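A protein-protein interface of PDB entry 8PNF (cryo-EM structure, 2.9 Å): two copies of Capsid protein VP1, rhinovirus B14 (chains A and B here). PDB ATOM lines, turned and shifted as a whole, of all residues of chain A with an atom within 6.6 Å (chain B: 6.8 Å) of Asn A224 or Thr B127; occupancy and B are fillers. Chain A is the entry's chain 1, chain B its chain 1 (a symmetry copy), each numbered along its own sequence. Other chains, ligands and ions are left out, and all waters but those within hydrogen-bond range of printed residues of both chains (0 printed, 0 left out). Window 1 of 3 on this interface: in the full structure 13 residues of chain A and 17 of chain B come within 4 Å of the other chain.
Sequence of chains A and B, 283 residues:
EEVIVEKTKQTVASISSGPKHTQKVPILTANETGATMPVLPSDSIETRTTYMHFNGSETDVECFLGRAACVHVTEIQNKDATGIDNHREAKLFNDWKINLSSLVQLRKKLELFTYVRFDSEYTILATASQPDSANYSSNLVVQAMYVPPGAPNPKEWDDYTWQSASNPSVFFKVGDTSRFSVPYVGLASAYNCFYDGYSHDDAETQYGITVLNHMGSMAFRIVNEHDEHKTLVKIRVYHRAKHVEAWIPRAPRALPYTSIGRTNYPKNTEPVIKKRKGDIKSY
Among the printed residues, pairs that only touch across the chains: Val A223 with Arg B236 (3.6 Å), Asn A224 with Thr B127 (3.97 Å), Asn A224 with Ala B128 (3.6 Å) and Glu A225 with Ser B129 (3.9 Å).
No position is printed for both chains. Of the 5 pairs that touch across the chains among the printed residues, none has its exchanged pair printed and touching as well.
Asn A224 touches just these residues of chain B: Thr B127 (3.97 Å) and Ala B128 (3.6 Å). Thr B127 touches just one residue of chain A: Asn A224 (3.97 Å). Of the printed residues of chain A, Ala B128 touches Asn A224 (3.6 Å). Leu B232 touches none of the printed residues of chain A. Printed residues of chain A within 4 Å of Lys B234: Glu A225 (3.2 Å).
Printed residues of chain B that touch a printed residue of chain A: Thr B127, Ala B128, Ser B129, Lys B234 and Arg B236. Of the 13 printed residues of chain A, 3 touch a printed residue of chain B. Hydrophobic or aromatic side chains of chain A that line the printed part of chain B: Val A223. Among the printed residues, Asp or Glu carboxylates within 4 Å of a Lys or Arg side-chain nitrogen of the other chain: Glu A225 with Lys B234.
NZ of Lys B234 lies within salt-bridge range of OE2 of Glu A225 (3.2 Å).
The side-chain amide oxygen of Asn A78 sits close to the backbone carbonyl oxygen of Asn A224 (2.9 Å). The side-chain amide nitrogen (ND2) of Asn A78 sits at hydrogen-bond distance from the backbone carbonyl oxygen (O) of Glu A225, at 2.5 Å. O of Val A141 lies within hydrogen-bond range of N of Val A223, 2.9 Å away. N of Val A141 sits at hydrogen-bond distance from OD1 of Asn A224 (3.0 Å). The backbone carbonyl oxygen of Thr B127 sits at hydrogen-bond distance from the backbone NH of Lys B234, at 2.8 Å. The backbone NH (N) of Leu B232 lies within hydrogen-bond range of the backbone carbonyl oxygen (O) of Ser B129.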
ATOM      1  N   ASN A  78      -4.827   6.768   7.774  1.00  0.00           N
ATOM      2  CA  ASN A  78      -4.209   5.704   8.554  1.00  0.00           C
ATOM      3  C   ASN A  78      -3.918   4.557   7.595  1.00  0.00           C
ATOM      4  O   ASN A  78      -4.711   3.622   7.463  1.00  0.00           O
ATOM      5  CB  ASN A  78      -5.133   5.272   9.694  1.00  0.00           C
ATOM      6  CG  ASN A  78      -4.466   4.329  10.662  1.00  0.00           C
ATOM      7  OD1 ASN A  78      -3.695   4.748  11.514  1.00  0.00           O
ATOM      8  ND2 ASN A  78      -4.779   3.047  10.549  1.00  0.00           N
ATOM      9  N   SER A 138     -12.609   1.296  11.210  1.00  0.00           N
ATOM     10  CA  SER A 138     -11.546   1.283  12.205  1.00  0.00           C
ATOM     11  C   SER A 138     -11.897   2.165  13.396  1.00  0.00           C
ATOM     12  O   SER A 138     -12.552   3.200  13.253  1.00  0.00           O
ATOM     13  CB  SER A 138     -10.233   1.746  11.581  1.00  0.00           C
ATOM     14  OG  SER A 138      -9.826   0.872  10.546  1.00  0.00           O
ATOM     15  N   ASN A 139     -11.467   1.734  14.579  1.00  0.00           N
ATOM     16  CA  ASN A 139     -11.678   2.477  15.820  1.00  0.00           C
ATOM     17  C   ASN A 139     -10.422   3.298  16.066  1.00  0.00           C
ATOM     18  O   ASN A 139      -9.477   2.849  16.712  1.00  0.00           O
ATOM     19  CB  ASN A 139     -11.971   1.525  16.970  1.00  0.00           C
ATOM     20  CG  ASN A 139     -12.652   2.208  18.136  1.00  0.00           C
ATOM     21  OD1 ASN A 139     -13.558   3.016  17.951  1.00  0.00           O
ATOM     22  ND2 ASN A 139     -12.217   1.883  19.350  1.00  0.00           N
ATOM     23  N   LEU A 140     -10.410   4.519  15.542  1.00  0.00           N
ATOM     24  CA  LEU A 140      -9.197   5.316  15.456  1.00  0.00           C
ATOM     25  C   LEU A 140      -9.161   6.406  16.516  1.00  0.00           C
ATOM     26  O   LEU A 140     -10.196   6.908  16.960  1.00  0.00           O
ATOM     27  CB  LEU A 140      -9.065   5.956  14.077  1.00  0.00           C
ATOM     28  CG  LEU A 140      -8.981   5.026  12.875  1.00  0.00           C
ATOM     29  CD1 LEU A 140      -9.034   5.852  11.619  1.00  0.00           C
ATOM     30  CD2 LEU A 140      -7.721   4.193  12.920  1.00  0.00           C
ATOM     31  N   VAL A 141      -7.945   6.774  16.907  1.00  0.00           N
ATOM     32  CA  VAL A 141      -7.695   7.828  17.881  1.00  0.00           C
ATOM     33  C   VAL A 141      -6.810   8.874  17.217  1.00  0.00           C
ATOM     34  O   VAL A 141      -5.790   8.532  16.610  1.00  0.00           O
ATOM     35  CB  VAL A 141      -7.038   7.269  19.161  1.00  0.00           C
ATOM     36  CG1 VAL A 141      -6.582   8.382  20.090  1.00  0.00           C
ATOM     37  CG2 VAL A 141      -7.995   6.348  19.887  1.00  0.00           C
ATOM     38  N   VAL A 142      -7.201  10.140  17.323  1.00  0.00           N
ATOM     39  CA  VAL A 142      -6.466  11.262  16.750  1.00  0.00           C
ATOM     40  C   VAL A 142      -5.702  11.978  17.854  1.00  0.00           C
ATOM     41  O   VAL A 142      -6.252  12.244  18.928  1.00  0.00           O
ATOM     42  CB  VAL A 142      -7.415  12.223  16.012  1.00  0.00           C
ATOM     43  CG1 VAL A 142      -6.686  13.448  15.513  1.00  0.00           C
ATOM     44  CG2 VAL A 142      -7.985  11.530  14.825  1.00  0.00           C
ATOM     45  N   TRP A 157       4.977  10.323  11.212  1.00  0.00           N
ATOM     46  CA  TRP A 157       3.861  10.115  12.123  1.00  0.00           C
ATOM     47  C   TRP A 157       4.292   9.413  13.406  1.00  0.00           C
ATOM     48  O   TRP A 157       3.654   9.602  14.444  1.00  0.00           O
ATOM     49  CB  TRP A 157       2.748   9.337  11.412  1.00  0.00           C
ATOM     50  CG  TRP A 157       2.952   7.854  11.364  1.00  0.00           C
ATOM     51  CD1 TRP A 157       3.606   7.150  10.402  1.00  0.00           C
ATOM     52  CD2 TRP A 157       2.487   6.893  12.318  1.00  0.00           C
ATOM     53  NE1 TRP A 157       3.589   5.812  10.700  1.00  0.00           N
ATOM     54  CE2 TRP A 157       2.910   5.628  11.874  1.00  0.00           C
ATOM     55  CE3 TRP A 157       1.768   6.983  13.512  1.00  0.00           C
ATOM     56  CZ2 TRP A 157       2.629   4.462  12.576  1.00  0.00           C
ATOM     57  CZ3 TRP A 157       1.495   5.829  14.208  1.00  0.00           C
ATOM     58  CH2 TRP A 157       1.920   4.584  13.738  1.00  0.00           C
ATOM     59  N   ARG A 221      -2.368  13.794  13.796  1.00  0.00           N
ATOM     60  CA  ARG A 221      -1.975  12.457  13.371  1.00  0.00           C
ATOM     61  C   ARG A 221      -3.004  11.466  13.890  1.00  0.00           C
ATOM     62  O   ARG A 221      -3.884  11.810  14.680  1.00  0.00           O
ATOM     63  CB  ARG A 221      -0.576  12.080  13.866  1.00  0.00           C
ATOM     64  CG  ARG A 221      -0.514  11.691  15.330  1.00  0.00           C
ATOM     65  CD  ARG A 221       0.754  10.929  15.628  1.00  0.00           C
ATOM     66  NE  ARG A 221       0.977  10.780  17.059  1.00  0.00           N
ATOM     67  CZ  ARG A 221       1.615   9.754  17.609  1.00  0.00           C
ATOM     68  NH1 ARG A 221       2.094   8.782  16.847  1.00  0.00           N
ATOM     69  NH2 ARG A 221       1.771   9.698  18.921  1.00  0.00           N
ATOM     70  N   ILE A 222      -2.891  10.226  13.427  1.00  0.00           N
ATOM     71  CA  ILE A 222      -3.656   9.111  13.968  1.00  0.00           C
ATOM     72  C   ILE A 222      -2.690   8.223  14.736  1.00  0.00           C
ATOM     73  O   ILE A 222      -1.686   7.761  14.182  1.00  0.00           O
ATOM     74  CB  ILE A 222      -4.386   8.329  12.866  1.00  0.00           C
ATOM     75  CG1 ILE A 222      -5.433   9.214  12.205  1.00  0.00           C
ATOM     76  CG2 ILE A 222      -5.076   7.113  13.444  1.00  0.00           C
ATOM     77  CD1 ILE A 222      -5.928   8.684  10.897  1.00  0.00           C
ATOM     78  N   VAL A 223      -2.991   7.999  16.016  1.00  0.00           N
ATOM     79  CA  VAL A 223      -2.114   7.232  16.895  1.00  0.00           C
ATOM     80  C   VAL A 223      -2.104   5.754  16.507  1.00  0.00           C
ATOM     81  O   VAL A 223      -1.099   5.058  16.707  1.00  0.00           O
ATOM     82  CB  VAL A 223      -2.556   7.466  18.354  1.00  0.00           C
ATOM     83  CG1 VAL A 223      -1.641   6.778  19.359  1.00  0.00           C
ATOM     84  CG2 VAL A 223      -2.612   8.947  18.639  1.00  0.00           C
ATOM     85  N   ASN A 224      -3.193   5.260  15.917  1.00  0.00           N
ATOM     86  CA  ASN A 224      -3.322   3.849  15.577  1.00  0.00           C
ATOM     87  C   ASN A 224      -2.369   3.462  14.451  1.00  0.00           C
ATOM     88  O   ASN A 224      -1.861   4.304  13.708  1.00  0.00           O
ATOM     89  CB  ASN A 224      -4.756   3.523  15.159  1.00  0.00           C
ATOM     90  CG  ASN A 224      -5.747   3.709  16.282  1.00  0.00           C
ATOM     91  OD1 ASN A 224      -5.746   4.735  16.952  1.00  0.00           O
ATOM     92  ND2 ASN A 224      -6.604   2.721  16.491  1.00  0.00           N
ATOM     93  N   GLU A 225      -2.114   2.161  14.346  1.00  0.00           N
ATOM     94  CA  GLU A 225      -1.307   1.621  13.267  1.00  0.00           C
ATOM     95  C   GLU A 225      -2.184   1.365  12.047  1.00  0.00           C
ATOM     96  O   GLU A 225      -3.374   1.685  12.024  1.00  0.00           O
ATOM     97  CB  GLU A 225      -0.598   0.345  13.711  1.00  0.00           C
ATOM     98  CG  GLU A 225       0.405   0.550  14.825  1.00  0.00           C
ATOM     99  CD  GLU A 225       1.793   0.867  14.314  1.00  0.00           C
ATOM    100  OE1 GLU A 225       2.048   0.669  13.110  1.00  0.00           O
ATOM    101  OE2 GLU A 225       2.632   1.318  15.118  1.00  0.00           O
ATOM    102  N   HIS A 226      -1.594   0.771  11.020  1.00  0.00           N
ATOM    103  CA  HIS A 226      -2.312   0.553   9.777  1.00  0.00           C
ATOM    104  C   HIS A 226      -3.124  -0.734   9.826  1.00  0.00           C
ATOM    105  O   HIS A 226      -2.764  -1.703  10.500  1.00  0.00           O
ATOM    106  CB  HIS A 226      -1.338   0.510   8.604  1.00  0.00           C
ATOM    107  CG  HIS A 226      -0.523  -0.742   8.538  1.00  0.00           C
ATOM    108  ND1 HIS A 226      -0.882  -1.821   7.761  1.00  0.00           N
ATOM    109  CD2 HIS A 226       0.631  -1.088   9.154  1.00  0.00           C
ATOM    110  CE1 HIS A 226       0.017  -2.778   7.900  1.00  0.00           C
ATOM    111  NE2 HIS A 226       0.945  -2.359   8.740  1.00  0.00           N
ATOM    112  N   ILE B  76       1.373  -5.913  22.909  1.00  0.00           N
ATOM    113  CA  ILE B  76       0.891  -7.270  23.138  1.00  0.00           C
ATOM    114  C   ILE B  76      -0.113  -7.616  22.050  1.00  0.00           C
ATOM    115  O   ILE B  76      -0.645  -6.727  21.382  1.00  0.00           O
ATOM    116  CB  ILE B  76       0.250  -7.425  24.527  1.00  0.00           C
ATOM    117  CG1 ILE B  76      -0.678  -6.251  24.817  1.00  0.00           C
ATOM    118  CG2 ILE B  76       1.306  -7.546  25.597  1.00  0.00           C
ATOM    119  CD1 ILE B  76      -1.461  -6.417  26.070  1.00  0.00           C
ATOM    120  N   LEU B 125      -2.797   4.083  27.685  1.00  0.00           N
ATOM    121  CA  LEU B 125      -3.633   4.103  26.494  1.00  0.00           C
ATOM    122  C   LEU B 125      -3.336   2.862  25.669  1.00  0.00           C
ATOM    123  O   LEU B 125      -2.171   2.526  25.445  1.00  0.00           O
ATOM    124  CB  LEU B 125      -3.380   5.370  25.677  1.00  0.00           C
ATOM    125  CG  LEU B 125      -4.010   5.498  24.292  1.00  0.00           C
ATOM    126  CD1 LEU B 125      -5.521   5.448  24.380  1.00  0.00           C
ATOM    127  CD2 LEU B 125      -3.565   6.788  23.633  1.00  0.00           C
ATOM    128  N   ALA B 126      -4.386   2.175  25.231  1.00  0.00           N
ATOM    129  CA  ALA B 126      -4.257   0.958  24.443  1.00  0.00           C
ATOM    130  C   ALA B 126      -5.013   1.128  23.137  1.00  0.00           C
ATOM    131  O   ALA B 126      -6.206   1.440  23.143  1.00  0.00           O
ATOM    132  CB  ALA B 126      -4.784  -0.254  25.210  1.00  0.00           C
ATOM    133  N   THR B 127      -4.315   0.929  22.021  1.00  0.00           N
ATOM    134  CA  THR B 127      -4.906   1.028  20.692  1.00  0.00           C
ATOM    135  C   THR B 127      -4.640  -0.276  19.960  1.00  0.00           C
ATOM    136  O   THR B 127      -3.533  -0.811  20.042  1.00  0.00           O
ATOM    137  CB  THR B 127      -4.325   2.211  19.906  1.00  0.00           C
ATOM    138  OG1 THR B 127      -2.904   2.072  19.815  1.00  0.00           O
ATOM    139  CG2 THR B 127      -4.657   3.534  20.575  1.00  0.00           C
ATOM    140  N   ALA B 128      -5.640  -0.784  19.250  1.00  0.00           N
ATOM    141  CA  ALA B 128      -5.483  -2.043  18.541  1.00  0.00           C
ATOM    142  C   ALA B 128      -5.258  -1.817  17.053  1.00  0.00           C
ATOM    143  O   ALA B 128      -5.439  -0.718  16.528  1.00  0.00           O
ATOM    144  CB  ALA B 128      -6.701  -2.944  18.728  1.00  0.00           C
ATOM    145  N   SER B 129      -4.847  -2.889  16.381  1.00  0.00           N
ATOM    146  CA  SER B 129      -4.704  -2.917  14.936  1.00  0.00           C
ATOM    147  C   SER B 129      -4.770  -4.363  14.479  1.00  0.00           C
ATOM    148  O   SER B 129      -4.312  -5.264  15.187  1.00  0.00           O
ATOM    149  CB  SER B 129      -3.385  -2.285  14.484  1.00  0.00           C
ATOM    150  OG  SER B 129      -2.293  -2.833  15.195  1.00  0.00           O
ATOM    151  N   VAL B 174      -9.774  -1.447  25.141  1.00  0.00           N
ATOM    152  CA  VAL B 174      -8.848  -0.956  24.128  1.00  0.00           C
ATOM    153  C   VAL B 174      -9.483   0.211  23.384  1.00  0.00           C
ATOM    154  O   VAL B 174     -10.605   0.104  22.875  1.00  0.00           O
ATOM    155  CB  VAL B 174      -8.464  -2.087  23.163  1.00  0.00           C
ATOM    156  CG1 VAL B 174      -7.783  -1.541  21.937  1.00  0.00           C
ATOM    157  CG2 VAL B 174      -7.572  -3.079  23.843  1.00  0.00           C
ATOM    158  N   GLY B 175      -8.764   1.327  23.309  1.00  0.00           N
ATOM    159  CA  GLY B 175      -9.294   2.521  22.690  1.00  0.00           C
ATOM    160  C   GLY B 175      -9.571   3.538  23.768  1.00  0.00           C
ATOM    161  O   GLY B 175      -9.732   4.732  23.507  1.00  0.00           O
ATOM    162  N   ASP B 176      -9.630   3.047  24.998  1.00  0.00           N
ATOM    163  CA  ASP B 176      -9.860   3.885  26.158  1.00  0.00           C
ATOM    164  C   ASP B 176      -8.557   4.062  26.928  1.00  0.00           C
ATOM    165  O   ASP B 176      -7.512   3.519  26.570  1.00  0.00           O
ATOM    166  CB  ASP B 176     -10.941   3.269  27.039  1.00  0.00           C
ATOM    167  CG  ASP B 176     -12.303   3.304  26.393  1.00  0.00           C
ATOM    168  OD1 ASP B 176     -12.558   4.223  25.591  1.00  0.00           O
ATOM    169  OD2 ASP B 176     -13.121   2.407  26.678  1.00  0.00           O
ATOM    170  N   LEU B 232      -3.043  -6.825  17.094  1.00  0.00           N
ATOM    171  CA  LEU B 232      -1.911  -6.280  17.838  1.00  0.00           C
ATOM    172  C   LEU B 232      -2.373  -5.077  18.650  1.00  0.00           C
ATOM    173  O   LEU B 232      -2.924  -4.125  18.092  1.00  0.00           O
ATOM    174  CB  LEU B 232      -0.795  -5.848  16.888  1.00  0.00           C
ATOM    175  CG  LEU B 232      -0.193  -6.781  15.840  1.00  0.00           C
ATOM    176  CD1 LEU B 232       1.017  -6.118  15.223  1.00  0.00           C
ATOM    177  CD2 LEU B 232       0.200  -8.102  16.435  1.00  0.00           C
ATOM    178  N   VAL B 233      -2.129  -5.102  19.955  1.00  0.00           N
ATOM    179  CA  VAL B 233      -2.514  -4.007  20.837  1.00  0.00           C
ATOM    180  C   VAL B 233      -1.247  -3.290  21.278  1.00  0.00           C
ATOM    181  O   VAL B 233      -0.353  -3.897  21.879  1.00  0.00           O
ATOM    182  CB  VAL B 233      -3.333  -4.508  22.038  1.00  0.00           C
ATOM    183  CG1 VAL B 233      -3.382  -3.463  23.139  1.00  0.00           C
ATOM    184  CG2 VAL B 233      -4.732  -4.854  21.594  1.00  0.00           C
ATOM    185  N   LYS B 234      -1.163  -2.003  20.966  1.00  0.00           N
ATOM    186  CA  LYS B 234      -0.034  -1.169  21.352  1.00  0.00           C
ATOM    187  C   LYS B 234      -0.420  -0.409  22.612  1.00  0.00           C
ATOM    188  O   LYS B 234      -1.506   0.170  22.682  1.00  0.00           O
ATOM    189  CB  LYS B 234       0.344  -0.205  20.232  1.00  0.00           C
ATOM    190  CG  LYS B 234       1.675   0.477  20.434  1.00  0.00           C
ATOM    191  CD  LYS B 234       2.822  -0.497  20.244  1.00  0.00           C
ATOM    192  CE  LYS B 234       3.002  -0.857  18.790  1.00  0.00           C
ATOM    193  NZ  LYS B 234       3.522   0.299  18.020  1.00  0.00           N
ATOM    194  N   ILE B 235       0.464  -0.414  23.602  1.00  0.00           N
ATOM    195  CA  ILE B 235       0.178   0.158  24.910  1.00  0.00           C
ATOM    196  C   ILE B 235       1.176   1.274  25.162  1.00  0.00           C
ATOM    197  O   ILE B 235       2.390   1.052  25.103  1.00  0.00           O
ATOM    198  CB  ILE B 235       0.236  -0.914  26.008  1.00  0.00           C
ATOM    199  CG1 ILE B 235      -1.043  -1.739  25.984  1.00  0.00           C
ATOM    200  CG2 ILE B 235       0.415  -0.294  27.379  1.00  0.00           C
ATOM    201  CD1 ILE B 235      -1.038  -2.848  26.964  1.00  0.00           C
ATOM    202  N   ARG B 236       0.670   2.475  25.422  1.00  0.00           N
ATOM    203  CA  ARG B 236       1.501   3.631  25.722  1.00  0.00           C
ATOM    204  C   ARG B 236       1.195   4.090  27.137  1.00  0.00           C
ATOM    205  O   ARG B 236       0.037   4.353  27.468  1.00  0.00           O
ATOM    206  CB  ARG B 236       1.262   4.764  24.726  1.00  0.00           C
ATOM    207  CG  ARG B 236       1.535   4.378  23.294  1.00  0.00           C
ATOM    208  CD  ARG B 236       1.204   5.500  22.340  1.00  0.00           C
ATOM    209  NE  ARG B 236       1.044   4.999  20.978  1.00  0.00           N
ATOM    210  CZ  ARG B 236       1.984   5.061  20.047  1.00  0.00           C
ATOM    211  NH1 ARG B 236       3.157   5.601  20.330  1.00  0.00           N
ATOM    212  NH2 ARG B 236       1.755   4.577  18.836  1.00  0.00           N
